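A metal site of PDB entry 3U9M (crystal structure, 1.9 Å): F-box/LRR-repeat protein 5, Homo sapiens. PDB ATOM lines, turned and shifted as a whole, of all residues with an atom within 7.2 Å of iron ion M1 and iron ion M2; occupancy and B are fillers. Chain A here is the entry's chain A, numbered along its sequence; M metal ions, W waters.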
ATOM      1  N   VAL A  10      15.589  20.277 -22.536  1.00  0.00           N
ATOM      2  CA  VAL A  10      14.507  21.247 -22.371  1.00  0.00           C
ATOM      3  C   VAL A  10      13.175  20.641 -21.913  1.00  0.00           C
ATOM      4  O   VAL A  10      12.189  21.369 -21.806  1.00  0.00           O
ATOM      5  CB  VAL A  10      14.261  22.048 -23.658  1.00  0.00           C
ATOM      6  CG1 VAL A  10      15.535  22.761 -24.094  1.00  0.00           C
ATOM      7  CG2 VAL A  10      13.705  21.145 -24.765  1.00  0.00           C
ATOM      8  N   PHE A  11      13.159  19.344 -21.646  1.00  0.00           N
ATOM      9  CA  PHE A  11      11.894  18.639 -21.371  1.00  0.00           C
ATOM     10  C   PHE A  11      11.835  17.894 -20.031  1.00  0.00           C
ATOM     11  O   PHE A  11      10.784  17.832 -19.399  1.00  0.00           O
ATOM     12  CB  PHE A  11      11.583  17.644 -22.501  1.00  0.00           C
ATOM     13  CG  PHE A  11      11.247  18.285 -23.809  1.00  0.00           C
ATOM     14  CD1 PHE A  11      10.138  19.129 -23.931  1.00  0.00           C
ATOM     15  CD2 PHE A  11      12.012  18.039 -24.935  1.00  0.00           C
ATOM     16  CE1 PHE A  11       9.823  19.717 -25.145  1.00  0.00           C
ATOM     17  CE2 PHE A  11      11.710  18.623 -26.154  1.00  0.00           C
ATOM     18  CZ  PHE A  11      10.604  19.470 -26.254  1.00  0.00           C
ATOM     19  N   PRO A  14      10.857  20.075 -16.487  1.00  0.00           N
ATOM     20  CA  PRO A  14       9.451  20.458 -16.567  1.00  0.00           C
ATOM     21  C   PRO A  14       8.524  19.240 -16.489  1.00  0.00           C
ATOM     22  O   PRO A  14       7.542  19.282 -15.745  1.00  0.00           O
ATOM     23  CB  PRO A  14       9.352  21.104 -17.954  1.00  0.00           C
ATOM     24  CG  PRO A  14      10.699  21.702 -18.146  1.00  0.00           C
ATOM     25  CD  PRO A  14      11.658  20.724 -17.543  1.00  0.00           C
ATOM     26  N   HIS A  15       8.846  18.196 -17.234  1.00  0.00           N
ATOM     27  CA  HIS A  15       8.046  16.967 -17.206  1.00  0.00           C
ATOM     28  C   HIS A  15       8.029  16.279 -15.841  1.00  0.00           C
ATOM     29  O   HIS A  15       7.061  15.599 -15.487  1.00  0.00           O
ATOM     30  CB  HIS A  15       8.518  15.992 -18.289  1.00  0.00           C
ATOM     31  CG  HIS A  15       8.163  16.420 -19.679  1.00  0.00           C
ATOM     32  ND1 HIS A  15       8.606  15.744 -20.800  1.00  0.00           N
ATOM     33  CD2 HIS A  15       7.416  17.447 -20.142  1.00  0.00           C
ATOM     34  CE1 HIS A  15       8.145  16.335 -21.884  1.00  0.00           C
ATOM     35  NE2 HIS A  15       7.414  17.378 -21.511  1.00  0.00           N
ATOM     36  N   MET A  18       5.304  18.067 -14.308  1.00  0.00           N
ATOM     37  CA  MET A  18       4.044  17.653 -14.922  1.00  0.00           C
ATOM     38  C   MET A  18       3.605  16.284 -14.424  1.00  0.00           C
ATOM     39  O   MET A  18       2.443  16.083 -14.062  1.00  0.00           O
ATOM     40  CB  MET A  18       4.141  17.676 -16.459  1.00  0.00           C
ATOM     41  CG  MET A  18       4.473  19.054 -17.040  1.00  0.00           C
ATOM     42  SD  MET A  18       3.438  20.378 -16.390  1.00  0.00           S
ATOM     43  CE  MET A  18       4.679  21.431 -15.631  1.00  0.00           C
ATOM     44  N   PHE A  54      -0.636  22.997 -16.661  1.00  0.00           N
ATOM     45  CA  PHE A  54      -0.356  22.217 -17.874  1.00  0.00           C
ATOM     46  C   PHE A  54      -0.397  23.131 -19.088  1.00  0.00           C
ATOM     47  O   PHE A  54       0.482  23.092 -19.956  1.00  0.00           O
ATOM     48  CB  PHE A  54      -1.392  21.107 -18.062  1.00  0.00           C
ATOM     49  CG  PHE A  54      -1.238  19.939 -17.123  1.00  0.00           C
ATOM     50  CD1 PHE A  54      -0.078  19.742 -16.389  1.00  0.00           C
ATOM     51  CD2 PHE A  54      -2.267  19.017 -16.979  1.00  0.00           C
ATOM     52  CE1 PHE A  54       0.042  18.663 -15.524  1.00  0.00           C
ATOM     53  CE2 PHE A  54      -2.155  17.928 -16.125  1.00  0.00           C
ATOM     54  CZ  PHE A  54      -1.001  17.751 -15.398  1.00  0.00           C
ATOM     55  N   HIS A  57       2.548  25.199 -19.268  1.00  0.00           N
ATOM     56  CA  HIS A  57       3.663  24.369 -19.719  1.00  0.00           C
ATOM     57  C   HIS A  57       3.699  24.243 -21.237  1.00  0.00           C
ATOM     58  O   HIS A  57       4.761  24.418 -21.856  1.00  0.00           O
ATOM     59  CB  HIS A  57       3.618  22.975 -19.076  1.00  0.00           C
ATOM     60  CG  HIS A  57       4.585  22.010 -19.671  1.00  0.00           C
ATOM     61  ND1 HIS A  57       5.941  22.067 -19.438  1.00  0.00           N
ATOM     62  CD2 HIS A  57       4.400  20.949 -20.506  1.00  0.00           C
ATOM     63  CE1 HIS A  57       6.549  21.094 -20.084  1.00  0.00           C
ATOM     64  NE2 HIS A  57       5.635  20.402 -20.745  1.00  0.00           N
ATOM     65  N   GLU A  58       2.559  23.940 -21.841  1.00  0.00           N
ATOM     66  CA  GLU A  58       2.471  23.805 -23.293  1.00  0.00           C
ATOM     67  C   GLU A  58       2.762  25.125 -23.985  1.00  0.00           C
ATOM     68  O   GLU A  58       3.435  25.166 -25.018  1.00  0.00           O
ATOM     69  CB  GLU A  58       1.090  23.282 -23.744  1.00  0.00           C
ATOM     70  CG  GLU A  58       0.656  21.966 -23.071  1.00  0.00           C
ATOM     71  CD  GLU A  58       1.626  20.839 -23.340  1.00  0.00           C
ATOM     72  OE1 GLU A  58       2.382  20.922 -24.320  1.00  0.00           O
ATOM     73  OE2 GLU A  58       1.642  19.872 -22.556  1.00  0.00           O
ATOM     74  N   GLN A  59       2.274  26.221 -23.407  1.00  0.00           N
ATOM     75  CA  GLN A  59       2.528  27.545 -23.973  1.00  0.00           C
ATOM     76  C   GLN A  59       4.006  27.907 -23.974  1.00  0.00           C
ATOM     77  O   GLN A  59       4.535  28.412 -24.968  1.00  0.00           O
ATOM     78  CB  GLN A  59       1.727  28.630 -23.234  1.00  0.00           C
ATOM     79  CG  GLN A  59       1.947  30.032 -23.796  1.00  0.00           C
ATOM     80  CD  GLN A  59       1.084  31.089 -23.128  1.00  0.00           C
ATOM     81  OE1 GLN A  59       0.057  30.791 -22.536  1.00  0.00           O
ATOM     82  NE2 GLN A  59       1.517  32.348 -23.228  1.00  0.00           N
ATOM     83  N   GLU A  61       6.508  25.857 -24.096  1.00  0.00           N
ATOM     84  CA  GLU A  61       7.079  25.048 -25.177  1.00  0.00           C
ATOM     85  C   GLU A  61       6.798  25.637 -26.563  1.00  0.00           C
ATOM     86  O   GLU A  61       7.708  25.722 -27.380  1.00  0.00           O
ATOM     87  CB  GLU A  61       6.576  23.615 -25.100  1.00  0.00           C
ATOM     88  CG  GLU A  61       7.097  22.875 -23.889  1.00  0.00           C
ATOM     89  CD  GLU A  61       6.508  21.495 -23.766  1.00  0.00           C
ATOM     90  OE1 GLU A  61       5.349  21.302 -24.194  1.00  0.00           O
ATOM     91  OE2 GLU A  61       7.212  20.595 -23.259  1.00  0.00           O
ATOM     92  N   ASN A  62       5.561  26.036 -26.824  1.00  0.00           N
ATOM     93  CA  ASN A  62       5.219  26.673 -28.090  1.00  0.00           C
ATOM     94  C   ASN A  62       6.016  27.965 -28.338  1.00  0.00           C
ATOM     95  O   ASN A  62       6.515  28.195 -29.438  1.00  0.00           O
ATOM     96  CB  ASN A  62       3.706  26.941 -28.186  1.00  0.00           C
ATOM     97  CG  ASN A  62       2.895  25.679 -28.425  1.00  0.00           C
ATOM     98  OD1 ASN A  62       3.371  24.708 -29.011  1.00  0.00           O
ATOM     99  ND2 ASN A  62       1.643  25.693 -27.977  1.00  0.00           N
ATOM    100  N   ILE A  66       9.143  25.122 -29.730  1.00  0.00           N
ATOM    101  CA  ILE A  66       8.587  24.601 -30.979  1.00  0.00           C
ATOM    102  C   ILE A  66       8.650  25.608 -32.121  1.00  0.00           C
ATOM    103  O   ILE A  66       8.998  25.247 -33.243  1.00  0.00           O
ATOM    104  CB  ILE A  66       7.122  24.127 -30.800  1.00  0.00           C
ATOM    105  CG1 ILE A  66       7.011  23.190 -29.591  1.00  0.00           C
ATOM    106  CG2 ILE A  66       6.620  23.458 -32.075  1.00  0.00           C
ATOM    107  CD1 ILE A  66       7.984  22.032 -29.627  1.00  0.00           C
ATOM    108  N   HIS A  80       3.429  20.016 -32.462  1.00  0.00           N
ATOM    109  CA  HIS A  80       3.280  19.969 -31.026  1.00  0.00           C
ATOM    110  C   HIS A  80       1.788  19.844 -30.732  1.00  0.00           C
ATOM    111  O   HIS A  80       1.047  20.811 -30.867  1.00  0.00           O
ATOM    112  CB  HIS A  80       3.867  21.216 -30.377  1.00  0.00           C
ATOM    113  CG  HIS A  80       3.787  21.205 -28.880  1.00  0.00           C
ATOM    114  ND1 HIS A  80       3.624  22.361 -28.144  1.00  0.00           N
ATOM    115  CD2 HIS A  80       3.862  20.190 -27.989  1.00  0.00           C
ATOM    116  CE1 HIS A  80       3.584  22.047 -26.863  1.00  0.00           C
ATOM    117  NE2 HIS A  80       3.731  20.740 -26.742  1.00  0.00           N
ATOM    118  N   SER A  81       1.359  18.644 -30.340  1.00  0.00           N
ATOM    119  CA  SER A  81      -0.065  18.363 -30.196  1.00  0.00           C
ATOM    120  C   SER A  81      -0.722  19.228 -29.124  1.00  0.00           C
ATOM    121  O   SER A  81      -0.046  19.816 -28.278  1.00  0.00           O
ATOM    122  CB  SER A  81      -0.314  16.879 -29.898  1.00  0.00           C
ATOM    123  OG  SER A  81      -0.202  16.610 -28.518  1.00  0.00           O
ATOM    124  N   ASP A  82      -2.053  19.285 -29.155  1.00  0.00           N
ATOM    125  CA  ASP A  82      -2.819  20.156 -28.275  1.00  0.00           C
ATOM    126  C   ASP A  82      -2.988  19.564 -26.875  1.00  0.00           C
ATOM    127  O   ASP A  82      -2.801  20.257 -25.869  1.00  0.00           O
ATOM    128  CB  ASP A  82      -4.192  20.429 -28.905  1.00  0.00           C
ATOM    129  CG  ASP A  82      -4.991  21.474 -28.158  1.00  0.00           C
ATOM    130  OD1 ASP A  82      -5.083  21.369 -26.916  1.00  0.00           O
ATOM    131  OD2 ASP A  82      -5.520  22.394 -28.802  1.00  0.00           O
ATOM    132  N   ASN A  83      -3.345  18.286 -26.810  1.00  0.00           N
ATOM    133  CA  ASN A  83      -3.713  17.619 -25.564  1.00  0.00           C
ATOM    134  C   ASN A  83      -5.101  18.035 -25.061  1.00  0.00           C
ATOM    135  O   ASN A  83      -5.557  17.574 -24.017  1.00  0.00           O
ATOM    136  CB  ASN A  83      -2.656  17.806 -24.479  1.00  0.00           C
ATOM    137  CG  ASN A  83      -1.428  16.915 -24.684  1.00  0.00           C
ATOM    138  OD1 ASN A  83      -1.461  15.973 -25.478  1.00  0.00           O
ATOM    139  ND2 ASN A  83      -0.352  17.213 -23.972  1.00  0.00           N
ATOM    140  N   PHE A 123      -1.550  12.384 -22.635  1.00  0.00           N
ATOM    141  CA  PHE A 123      -0.515  13.261 -22.109  1.00  0.00           C
ATOM    142  C   PHE A 123       0.834  12.561 -21.941  1.00  0.00           C
ATOM    143  O   PHE A 123       1.865  13.144 -22.243  1.00  0.00           O
ATOM    144  CB  PHE A 123      -0.973  13.876 -20.775  1.00  0.00           C
ATOM    145  CG  PHE A 123      -0.079  14.993 -20.272  1.00  0.00           C
ATOM    146  CD1 PHE A 123       0.726  15.729 -21.139  1.00  0.00           C
ATOM    147  CD2 PHE A 123      -0.063  15.323 -18.928  1.00  0.00           C
ATOM    148  CE1 PHE A 123       1.523  16.747 -20.672  1.00  0.00           C
ATOM    149  CE2 PHE A 123       0.754  16.348 -18.455  1.00  0.00           C
ATOM    150  CZ  PHE A 123       1.535  17.057 -19.325  1.00  0.00           C
ATOM    151  N   HIS A 126       2.617  12.002 -25.181  1.00  0.00           N
ATOM    152  CA  HIS A 126       2.929  13.346 -25.665  1.00  0.00           C
ATOM    153  C   HIS A 126       4.278  13.826 -25.119  1.00  0.00           C
ATOM    154  O   HIS A 126       5.157  14.244 -25.874  1.00  0.00           O
ATOM    155  CB  HIS A 126       1.833  14.315 -25.213  1.00  0.00           C
ATOM    156  CG  HIS A 126       2.111  15.737 -25.553  1.00  0.00           C
ATOM    157  ND1 HIS A 126       1.568  16.350 -26.669  1.00  0.00           N
ATOM    158  CD2 HIS A 126       2.865  16.679 -24.945  1.00  0.00           C
ATOM    159  CE1 HIS A 126       1.983  17.609 -26.722  1.00  0.00           C
ATOM    160  NE2 HIS A 126       2.769  17.832 -25.677  1.00  0.00           N
ATOM    161  N   MET A 127       4.416  13.779 -23.808  1.00  0.00           N
ATOM    162  CA  MET A 127       5.658  14.159 -23.161  1.00  0.00           C
ATOM    163  C   MET A 127       6.808  13.296 -23.658  1.00  0.00           C
ATOM    164  O   MET A 127       7.879  13.796 -23.983  1.00  0.00           O
ATOM    165  CB  MET A 127       5.501  14.032 -21.647  1.00  0.00           C
ATOM    166  CG  MET A 127       4.645  15.130 -21.039  1.00  0.00           C
ATOM    167  SD  MET A 127       4.750  15.185 -19.240  1.00  0.00           S
ATOM    168  CE  MET A 127       3.793  13.722 -18.810  1.00  0.00           C
ATOM    169  N   LYS A 128       6.570  11.989 -23.717  1.00  0.00           N
ATOM    170  CA  LYS A 128       7.584  11.037 -24.147  1.00  0.00           C
ATOM    171  C   LYS A 128       8.083  11.349 -25.556  1.00  0.00           C
ATOM    172  O   LYS A 128       9.278  11.246 -25.834  1.00  0.00           O
ATOM    173  CB  LYS A 128       7.022   9.614 -24.082  1.00  0.00           C
ATOM    174  CG  LYS A 128       8.028   8.525 -24.401  1.00  0.00           C
ATOM    175  CD  LYS A 128       7.326   7.184 -24.531  1.00  0.00           C
ATOM    176  CE  LYS A 128       8.279   6.111 -25.045  1.00  0.00           C
ATOM    177  NZ  LYS A 128       7.545   4.902 -25.462  1.00  0.00           N
ATOM    178  N   GLU A 130       8.174  14.262 -26.997  1.00  0.00           N
ATOM    179  CA  GLU A 130       9.037  15.423 -26.903  1.00  0.00           C
ATOM    180  C   GLU A 130      10.447  14.998 -26.510  1.00  0.00           C
ATOM    181  O   GLU A 130      11.423  15.438 -27.116  1.00  0.00           O
ATOM    182  CB  GLU A 130       8.465  16.425 -25.915  1.00  0.00           C
ATOM    183  CG  GLU A 130       7.223  17.099 -26.428  1.00  0.00           C
ATOM    184  CD  GLU A 130       6.497  17.854 -25.359  1.00  0.00           C
ATOM    185  OE1 GLU A 130       6.760  17.624 -24.160  1.00  0.00           O
ATOM    186  OE2 GLU A 130       5.663  18.697 -25.718  1.00  0.00           O
ATOM    187  N   GLU A 131      10.539  14.126 -25.523  1.00  0.00           N
ATOM    188  CA  GLU A 131      11.837  13.686 -25.015  1.00  0.00           C
ATOM    189  C   GLU A 131      12.581  12.804 -26.010  1.00  0.00           C
ATOM    190  O   GLU A 131      13.799  12.885 -26.111  1.00  0.00           O
ATOM    191  CB  GLU A 131      11.659  12.930 -23.705  1.00  0.00           C
ATOM    192  CG  GLU A 131      11.167  13.804 -22.555  1.00  0.00           C
ATOM    193  CD  GLU A 131      10.505  12.988 -21.470  1.00  0.00           C
ATOM    194  OE1 GLU A 131      10.792  11.774 -21.371  1.00  0.00           O
ATOM    195  OE2 GLU A 131       9.679  13.544 -20.720  1.00  0.00           O
ATOM    196  N   PHE A 134      11.614  15.183 -30.292  1.00  0.00           N
ATOM    197  CA  PHE A 134      11.937  16.605 -30.410  1.00  0.00           C
ATOM    198  C   PHE A 134      13.338  16.956 -29.906  1.00  0.00           C
ATOM    199  O   PHE A 134      14.044  17.730 -30.557  1.00  0.00           O
ATOM    200  CB  PHE A 134      10.878  17.465 -29.728  1.00  0.00           C
ATOM    201  CG  PHE A 134       9.544  17.444 -30.426  1.00  0.00           C
ATOM    202  CD1 PHE A 134       9.469  17.450 -31.804  1.00  0.00           C
ATOM    203  CD2 PHE A 134       8.370  17.409 -29.691  1.00  0.00           C
ATOM    204  CE1 PHE A 134       8.243  17.415 -32.450  1.00  0.00           C
ATOM    205  CE2 PHE A 134       7.133  17.388 -30.333  1.00  0.00           C
ATOM    206  CZ  PHE A 134       7.077  17.390 -31.704  1.00  0.00           C
ATOM    207  N   HIS A 158       9.294  28.232 -16.107  1.00  0.00           N
ATOM    208  CA  HIS A 158       8.625  27.252 -15.261  1.00  0.00           C
ATOM    209  C   HIS A 158       8.796  27.630 -13.796  1.00  0.00           C
ATOM    210  O   HIS A 158       7.941  27.318 -12.979  1.00  0.00           O
ATOM    211  CB  HIS A 158       9.147  25.841 -15.536  1.00  0.00           C
ATOM    212  CG  HIS A 158       8.555  25.218 -16.756  1.00  0.00           C
ATOM    213  ND1 HIS A 158       9.035  25.459 -18.027  1.00  0.00           N
ATOM    214  CD2 HIS A 158       7.509  24.373 -16.903  1.00  0.00           C
ATOM    215  CE1 HIS A 158       8.314  24.783 -18.904  1.00  0.00           C
ATOM    216  NE2 HIS A 158       7.383  24.115 -18.247  1.00  0.00           N
HETATM  217 FE    FE M   1       4.052  19.619 -24.900  1.00  0.00          FE
HETATM  218 FE    FE M   2       6.124  18.926 -22.477  1.00  0.00          FE
HETATM  219  O   HOH W   1       4.125  18.499 -23.027  1.00  0.00           O
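Of the 24 residues printed, 5 come within 4 Å of iron ion M1. Along chain A the residues within 4 Å of iron ion M1 span positions 58 to 130.
The backbone carbonyl oxygen (O) of Glu 58 sits close to the side-chain amide nitrogen (ND2) of Asn 62 (3.5 Å). The backbone carbonyl oxygen (O) of Glu 61 lies within hydrogen-bond range of the backbone NH (N) of Ile 66, 2.8 Å away. A ring nitrogen (ND1) of His 15 lies within hydrogen-bond range of the side-chain carboxylate (OE2) of Glu 131. ND1 of His 126 is in hydrogen-bond range of OD1 of Asn 83, at 3.3 Å. The side-chain hydroxyl of Ser 81 is in hydrogen-bond range of a ring nitrogen (ND1) of His 126, 2.6 Å away. O of Phe 11 lies close to ND1 of His 15, at 3.3 Å. A ring nitrogen (ND1) of His 80 is in hydrogen-bond range of the side-chain amide oxygen (OD1) of Asn 62 (2.5 Å). A ring nitrogen (ND1) of His 57 is in hydrogen-bond range of a ring nitrogen (NE2) of His 158, at 2.8 Å.
Four residues have an atom within 4 Å of iron ion M2: His 15, His 57, Glu 61 and Glu 130. Along chain A the residues within 4 Å of iron ion M2 span positions 15 to 130.
Iron ion M1 is bound by OE2 of Glu 130, at 2.0 Å. Iron ion M1 is bound by a ring nitrogen (NE2) of His 80. Water W1 binds iron ion M1. Iron ion M1 is bound by the side-chain carboxylate (OE1) of Glu 58, at 2.2 Å. OE1 of Glu 61 binds iron ion M1 (2.2 Å). Iron ion M1 is bound by NE2 of His 126 (2.3 Å).
Iron ion M2 is bound by water W1. OE2 of Glu 61 is bound to iron ion M2. The side-chain carboxylate (OE1) of Glu 130 binds iron ion M2 (2.2 Å). Iron ion M2 is bound by a ring nitrogen (NE2) of His 15 (2.2 Å). Iron ion M2 is bound by a ring nitrogen (NE2) of His 57 (2.3 Å). Iron ion M2 has five donor atoms within binding distance.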
